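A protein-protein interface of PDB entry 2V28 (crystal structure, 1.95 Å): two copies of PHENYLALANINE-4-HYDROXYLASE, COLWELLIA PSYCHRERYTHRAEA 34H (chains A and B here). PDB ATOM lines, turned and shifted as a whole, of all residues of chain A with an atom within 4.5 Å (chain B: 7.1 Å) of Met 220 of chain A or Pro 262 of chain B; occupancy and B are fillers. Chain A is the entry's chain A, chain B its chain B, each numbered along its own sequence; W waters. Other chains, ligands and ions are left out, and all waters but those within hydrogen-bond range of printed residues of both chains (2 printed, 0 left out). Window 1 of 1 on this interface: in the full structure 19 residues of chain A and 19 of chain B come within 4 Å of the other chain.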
ATOM      1  N   GLY A 189     -15.928  -8.095 -15.367  1.00  0.00           N
ATOM      2  CA  GLY A 189     -17.164  -7.806 -16.101  1.00  0.00           C
ATOM      3  C   GLY A 189     -17.876  -6.548 -15.624  1.00  0.00           C
ATOM      4  O   GLY A 189     -18.300  -5.721 -16.440  1.00  0.00           O
ATOM      5  N   GLU A 190     -18.012  -6.386 -14.311  1.00  0.00           N
ATOM      6  CA  GLU A 190     -18.558  -5.111 -13.785  1.00  0.00           C
ATOM      7  C   GLU A 190     -17.650  -3.927 -14.084  1.00  0.00           C
ATOM      8  O   GLU A 190     -18.119  -2.820 -14.301  1.00  0.00           O
ATOM      9  CB  GLU A 190     -18.784  -5.171 -12.278  1.00  0.00           C
ATOM     10  CG  GLU A 190     -19.763  -6.224 -11.838  1.00  0.00           C
ATOM     11  CD  GLU A 190     -21.202  -5.992 -12.333  1.00  0.00           C
ATOM     12  OE1 GLU A 190     -21.525  -4.906 -12.870  1.00  0.00           O
ATOM     13  OE2 GLU A 190     -22.026  -6.918 -12.176  1.00  0.00           O
ATOM     14  N   TYR A 193     -17.922  -2.965 -17.847  1.00  0.00           N
ATOM     15  CA  TYR A 193     -19.207  -2.364 -18.126  1.00  0.00           C
ATOM     16  C   TYR A 193     -19.312  -0.958 -17.543  1.00  0.00           C
ATOM     17  O   TYR A 193     -19.702  -0.059 -18.253  1.00  0.00           O
ATOM     18  CB  TYR A 193     -20.334  -3.257 -17.643  1.00  0.00           C
ATOM     19  CG  TYR A 193     -21.716  -2.726 -17.839  1.00  0.00           C
ATOM     20  CD1 TYR A 193     -22.428  -2.977 -19.023  1.00  0.00           C
ATOM     21  CD2 TYR A 193     -22.351  -2.040 -16.817  1.00  0.00           C
ATOM     22  CE1 TYR A 193     -23.721  -2.520 -19.177  1.00  0.00           C
ATOM     23  CE2 TYR A 193     -23.628  -1.588 -16.959  1.00  0.00           C
ATOM     24  CZ  TYR A 193     -24.307  -1.823 -18.136  1.00  0.00           C
ATOM     25  OH  TYR A 193     -25.583  -1.346 -18.249  1.00  0.00           O
ATOM     26  N   ILE A 219     -29.026  -7.725 -12.882  1.00  0.00           N
ATOM     27  CA  ILE A 219     -28.964  -7.146 -14.218  1.00  0.00           C
ATOM     28  C   ILE A 219     -27.757  -6.218 -14.323  1.00  0.00           C
ATOM     29  O   ILE A 219     -27.198  -5.798 -13.293  1.00  0.00           O
ATOM     30  CB  ILE A 219     -30.265  -6.380 -14.614  1.00  0.00           C
ATOM     31  CG1 ILE A 219     -30.456  -5.085 -13.776  1.00  0.00           C
ATOM     32  CG2 ILE A 219     -31.469  -7.288 -14.525  1.00  0.00           C
ATOM     33  CD1 ILE A 219     -31.556  -4.144 -14.310  1.00  0.00           C
ATOM     34  N   MET A 220     -27.369  -5.904 -15.555  1.00  0.00           N
ATOM     35  CA  MET A 220     -26.384  -4.888 -15.791  1.00  0.00           C
ATOM     36  C   MET A 220     -27.034  -3.545 -15.479  1.00  0.00           C
ATOM     37  O   MET A 220     -28.108  -3.232 -15.988  1.00  0.00           O
ATOM     38  CB  MET A 220     -25.859  -4.921 -17.251  1.00  0.00           C
ATOM     39  CG  MET A 220     -25.297  -6.295 -17.722  1.00  0.00           C
ATOM     40  SD  MET A 220     -24.110  -7.022 -16.598  1.00  0.00           S
ATOM     41  CE  MET A 220     -22.707  -5.950 -16.808  1.00  0.00           C
ATOM     42  N   GLN A 221     -26.370  -2.755 -14.649  1.00  0.00           N
ATOM     43  CA  GLN A 221     -26.983  -1.544 -14.101  1.00  0.00           C
ATOM     44  C   GLN A 221     -27.190  -0.451 -15.149  1.00  0.00           C
ATOM     45  O   GLN A 221     -26.224  -0.056 -15.789  1.00  0.00           O
ATOM     46  CB  GLN A 221     -26.106  -1.016 -12.973  1.00  0.00           C
ATOM     47  CG  GLN A 221     -26.022  -1.914 -11.773  1.00  0.00           C
ATOM     48  CD  GLN A 221     -27.361  -2.305 -11.253  1.00  0.00           C
ATOM     49  OE1 GLN A 221     -28.078  -1.471 -10.711  1.00  0.00           O
ATOM     50  NE2 GLN A 221     -27.724  -3.593 -11.405  1.00  0.00           N
ATOM     51  N   PRO A 222     -28.451   0.045 -15.337  1.00  0.00           N
ATOM     52  CA  PRO A 222     -28.645   1.108 -16.297  1.00  0.00           C
ATOM     53  C   PRO A 222     -28.259   2.470 -15.796  1.00  0.00           C
ATOM     54  O   PRO A 222     -28.118   3.397 -16.608  1.00  0.00           O
ATOM     55  CB  PRO A 222     -30.155   1.068 -16.586  1.00  0.00           C
ATOM     56  CG  PRO A 222     -30.762   0.412 -15.416  1.00  0.00           C
ATOM     57  CD  PRO A 222     -29.719  -0.405 -14.735  1.00  0.00           C
ATOM     58  N   ARG B 216     -31.091 -15.777 -21.453  1.00  0.00           N
ATOM     59  CA  ARG B 216     -31.983 -15.582 -20.318  1.00  0.00           C
ATOM     60  C   ARG B 216     -33.070 -14.636 -20.792  1.00  0.00           C
ATOM     61  O   ARG B 216     -32.810 -13.713 -21.569  1.00  0.00           O
ATOM     62  CB  ARG B 216     -31.250 -14.946 -19.117  1.00  0.00           C
ATOM     63  CG  ARG B 216     -30.027 -15.706 -18.593  1.00  0.00           C
ATOM     64  CD  ARG B 216     -30.431 -17.009 -17.903  1.00  0.00           C
ATOM     65  NE  ARG B 216     -29.254 -17.784 -17.505  1.00  0.00           N
ATOM     66  CZ  ARG B 216     -28.726 -18.797 -18.202  1.00  0.00           C
ATOM     67  NH1 ARG B 216     -29.263 -19.189 -19.353  1.00  0.00           N
ATOM     68  NH2 ARG B 216     -27.638 -19.416 -17.740  1.00  0.00           N
ATOM     69  N   ILE B 219     -33.546 -10.474 -19.192  1.00  0.00           N
ATOM     70  CA  ILE B 219     -32.459  -9.501 -19.309  1.00  0.00           C
ATOM     71  C   ILE B 219     -32.455  -8.819 -20.678  1.00  0.00           C
ATOM     72  O   ILE B 219     -33.105  -9.283 -21.637  1.00  0.00           O
ATOM     73  CB  ILE B 219     -31.049 -10.108 -19.011  1.00  0.00           C
ATOM     74  CG1 ILE B 219     -30.681 -11.219 -20.019  1.00  0.00           C
ATOM     75  CG2 ILE B 219     -30.968 -10.585 -17.552  1.00  0.00           C
ATOM     76  CD1 ILE B 219     -29.200 -11.576 -20.092  1.00  0.00           C
ATOM     77  N   MET B 220     -31.726  -7.718 -20.775  1.00  0.00           N
ATOM     78  CA  MET B 220     -31.471  -7.131 -22.079  1.00  0.00           C
ATOM     79  C   MET B 220     -30.555  -8.099 -22.803  1.00  0.00           C
ATOM     80  O   MET B 220     -29.523  -8.514 -22.257  1.00  0.00           O
ATOM     81  CB  MET B 220     -30.833  -5.744 -21.959  1.00  0.00           C
ATOM     82  CG  MET B 220     -31.733  -4.709 -21.240  1.00  0.00           C
ATOM     83  SD  MET B 220     -33.524  -4.692 -21.639  1.00  0.00           S
ATOM     84  CE  MET B 220     -33.476  -4.082 -23.314  1.00  0.00           C
ATOM     85  N   GLN B 221     -30.966  -8.488 -24.012  1.00  0.00           N
ATOM     86  CA  GLN B 221     -30.237  -9.484 -24.802  1.00  0.00           C
ATOM     87  C   GLN B 221     -28.883  -8.978 -25.257  1.00  0.00           C
ATOM     88  O   GLN B 221     -28.790  -7.959 -25.944  1.00  0.00           O
ATOM     89  CB  GLN B 221     -31.063  -9.957 -26.000  1.00  0.00           C
ATOM     90  CG  GLN B 221     -32.374 -10.612 -25.581  1.00  0.00           C
ATOM     91  CD  GLN B 221     -32.153 -11.809 -24.698  1.00  0.00           C
ATOM     92  OE1 GLN B 221     -31.624 -12.815 -25.140  1.00  0.00           O
ATOM     93  NE2 GLN B 221     -32.562 -11.709 -23.432  1.00  0.00           N
ATOM     94  N   PRO B 222     -27.819  -9.687 -24.853  1.00  0.00           N
ATOM     95  CA  PRO B 222     -26.455  -9.270 -25.222  1.00  0.00           C
ATOM     96  C   PRO B 222     -26.060  -9.686 -26.652  1.00  0.00           C
ATOM     97  O   PRO B 222     -25.145  -9.092 -27.221  1.00  0.00           O
ATOM     98  CB  PRO B 222     -25.571  -9.931 -24.148  1.00  0.00           C
ATOM     99  CG  PRO B 222     -26.380 -11.152 -23.649  1.00  0.00           C
ATOM    100  CD  PRO B 222     -27.857 -10.894 -23.996  1.00  0.00           C
ATOM    101  N   ALA B 259     -21.167 -18.444 -21.839  1.00  0.00           N
ATOM    102  CA  ALA B 259     -22.211 -17.448 -21.573  1.00  0.00           C
ATOM    103  C   ALA B 259     -21.591 -16.058 -21.547  1.00  0.00           C
ATOM    104  O   ALA B 259     -20.508 -15.886 -20.994  1.00  0.00           O
ATOM    105  CB  ALA B 259     -22.852 -17.741 -20.239  1.00  0.00           C
ATOM    106  N   LYS B 260     -22.264 -15.070 -22.130  1.00  0.00           N
ATOM    107  CA  LYS B 260     -21.839 -13.655 -21.933  1.00  0.00           C
ATOM    108  C   LYS B 260     -22.063 -13.282 -20.476  1.00  0.00           C
ATOM    109  O   LYS B 260     -22.933 -13.857 -19.821  1.00  0.00           O
ATOM    110  CB  LYS B 260     -22.681 -12.718 -22.764  1.00  0.00           C
ATOM    111  CG  LYS B 260     -22.580 -12.963 -24.222  1.00  0.00           C
ATOM    112  CD  LYS B 260     -21.373 -12.320 -24.808  1.00  0.00           C
ATOM    113  CE  LYS B 260     -21.464 -12.541 -26.285  1.00  0.00           C
ATOM    114  NZ  LYS B 260     -20.732 -11.509 -27.040  1.00  0.00           N
ATOM    115  N   PHE B 261     -21.269 -12.337 -19.974  1.00  0.00           N
ATOM    116  CA  PHE B 261     -21.304 -11.979 -18.565  1.00  0.00           C
ATOM    117  C   PHE B 261     -22.723 -11.680 -18.035  1.00  0.00           C
ATOM    118  O   PHE B 261     -23.059 -12.116 -16.917  1.00  0.00           O
ATOM    119  CB  PHE B 261     -20.342 -10.808 -18.283  1.00  0.00           C
ATOM    120  CG  PHE B 261     -20.359 -10.339 -16.853  1.00  0.00           C
ATOM    121  CD1 PHE B 261     -19.664 -11.026 -15.884  1.00  0.00           C
ATOM    122  CD2 PHE B 261     -21.052  -9.183 -16.488  1.00  0.00           C
ATOM    123  CE1 PHE B 261     -19.657 -10.586 -14.549  1.00  0.00           C
ATOM    124  CE2 PHE B 261     -21.035  -8.734 -15.170  1.00  0.00           C
ATOM    125  CZ  PHE B 261     -20.338  -9.451 -14.199  1.00  0.00           C
ATOM    126  N   PRO B 262     -23.575 -10.976 -18.831  1.00  0.00           N
ATOM    127  CA  PRO B 262     -24.901 -10.717 -18.278  1.00  0.00           C
ATOM    128  C   PRO B 262     -25.770 -11.968 -18.139  1.00  0.00           C
ATOM    129  O   PRO B 262     -26.627 -11.977 -17.288  1.00  0.00           O
ATOM    130  CB  PRO B 262     -25.518  -9.731 -19.267  1.00  0.00           C
ATOM    131  CG  PRO B 262     -24.375  -9.191 -20.054  1.00  0.00           C
ATOM    132  CD  PRO B 262     -23.448 -10.361 -20.166  1.00  0.00           C
ATOM    133  N   VAL B 263     -25.511 -13.012 -18.934  1.00  0.00           N
ATOM    134  CA  VAL B 263     -26.180 -14.328 -18.769  1.00  0.00           C
ATOM    135  C   VAL B 263     -25.697 -15.035 -17.494  1.00  0.00           C
ATOM    136  O   VAL B 263     -26.493 -15.478 -16.678  1.00  0.00           O
ATOM    137  CB  VAL B 263     -25.979 -15.204 -20.040  1.00  0.00           C
ATOM    138  CG1 VAL B 263     -26.550 -16.634 -19.870  1.00  0.00           C
ATOM    139  CG2 VAL B 263     -26.607 -14.501 -21.230  1.00  0.00           C
ATOM    140  N   LYS B 264     -24.386 -15.108 -17.321  1.00  0.00           N
ATOM    141  CA  LYS B 264     -23.759 -15.641 -16.106  1.00  0.00           C
ATOM    142  C   LYS B 264     -24.343 -15.001 -14.845  1.00  0.00           C
ATOM    143  O   LYS B 264     -24.715 -15.693 -13.881  1.00  0.00           O
ATOM    144  CB  LYS B 264     -22.244 -15.409 -16.165  1.00  0.00           C
ATOM    145  CG  LYS B 264     -21.495 -16.320 -17.135  1.00  0.00           C
ATOM    146  CD  LYS B 264     -19.978 -16.135 -16.990  1.00  0.00           C
ATOM    147  CE  LYS B 264     -19.227 -16.963 -18.042  1.00  0.00           C
ATOM    148  NZ  LYS B 264     -17.822 -16.472 -18.280  1.00  0.00           N
ATOM    149  N   LYS B 265     -24.398 -13.668 -14.869  1.00  0.00           N
ATOM    150  CA  LYS B 265     -24.996 -12.864 -13.808  1.00  0.00           C
ATOM    151  C   LYS B 265     -26.479 -13.173 -13.507  1.00  0.00           C
ATOM    152  O   LYS B 265     -26.891 -13.134 -12.359  1.00  0.00           O
ATOM    153  CB  LYS B 265     -24.850 -11.390 -14.191  1.00  0.00           C
ATOM    154  CG  LYS B 265     -25.034 -10.463 -13.061  1.00  0.00           C
ATOM    155  CD  LYS B 265     -24.686  -9.049 -13.481  1.00  0.00           C
ATOM    156  CE  LYS B 265     -24.860  -8.128 -12.297  1.00  0.00           C
ATOM    157  NZ  LYS B 265     -24.835  -6.700 -12.737  1.00  0.00           N
ATOM    158  N   ALA B 266     -27.279 -13.458 -14.528  1.00  0.00           N
ATOM    159  CA  ALA B 266     -28.733 -13.634 -14.339  1.00  0.00           C
ATOM    160  C   ALA B 266     -29.160 -14.985 -13.734  1.00  0.00           C
ATOM    161  O   ALA B 266     -28.625 -16.039 -14.073  1.00  0.00           O
ATOM    162  CB  ALA B 266     -29.489 -13.346 -15.632  1.00  0.00           C
ATOM    163  N   SER B 267     -30.131 -14.932 -12.822  1.00  0.00           N
ATOM    164  CA  SER B 267     -30.493 -16.087 -11.981  1.00  0.00           C
ATOM    165  C   SER B 267     -31.381 -17.086 -12.730  1.00  0.00           C
ATOM    166  O   SER B 267     -31.450 -17.059 -13.969  1.00  0.00           O
ATOM    167  CB  SER B 267     -31.168 -15.611 -10.686  1.00  0.00           C
ATOM    168  OG  SER B 267     -30.348 -14.661  -9.996  1.00  0.00           O
HETATM  169  O   HOH W   1     -23.749  -3.651 -13.791  1.00  0.00           O
HETATM  170  O   HOH W   2     -25.619  -6.052 -10.120  1.00  0.00           O
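4 positions are printed for both chains. Of the 7 pairs that touch across the chains among the printed residues, none has its exchanged pair printed and touching as well.
OE2 of Glu 190 of chain A lies within salt-bridge range of NZ of Lys 265 of chain B, 2.9 Å away. O of Ile 219 of chain A lies within hydrogen-bond range of NZ of Lys 265 of chain B (2.6 Å).
Gly 189 of chain A touches Phe 261 of chain B (C to CE2, 3.9 Å). Glu 190 of chain A touches Phe 261 of chain B. Met 220 of chain A touches Phe 261 of chain B. CG of Met 220 of chain A touches CB of Pro 262 of chain B, 3.8 Å away. Met 220 of chain A touches Lys 265 of chain B (SD to CD, 3.8 Å).
Printed residues of chain B within 4 Å of Gly 189 of chain A: Phe 261 (3.9 Å). Of the printed residues of chain B, Glu 190 of chain A touches Phe 261 and Lys 265. Printed residues of chain B within 4 Å of Ile 219 of chain A: Lys 265 (2.6 Å). Of the printed residues of chain A, Phe 261 of chain B touches Gly 189, Glu 190 and Met 220. Of the printed residues of chain A, Pro 262 of chain B touches Met 220. Of the printed residues of chain A, Lys 265 of chain B touches Glu 190, Ile 219 and Met 220. The nearest printed residue of chain B that does not touch Glu 190 of chain A is Pro 262 of chain B (7.7 Å).
Water W1 lies within hydrogen-bond range of the side-chain carboxylate of Glu 190 of chain A, the backbone NH of Gln 221 of chain A and the side-chain amino group of Lys 265 of chain B. Water W2 bridges NZ of Lys 265 of chain B (2.8 Å) and NE2 of Gln 221 of chain A (3.5 Å).
Printed residues of chain A that touch a printed residue of chain B: Gly 189, Glu 190, Ile 219 and Met 220. Hydrophobic or aromatic side chains of chain A within 4 Å of the printed part of chain B: Met 220. Of the 14 printed residues of chain B, 3 touch a printed residue of chain A. Printed residues of chain B that touch a printed residue of chain A: Phe 261, Pro 262 and Lys 265. Among the printed residues, Asp or Glu carboxylates within 4 Å of a Lys or Arg side-chain nitrogen of the other chain: Glu 190 of chain A with Lys 265 of chain B.
O of Ile 219 of chain A sits at hydrogen-bond distance from NE2 of Gln 221 of chain A, 3.0 Å away.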
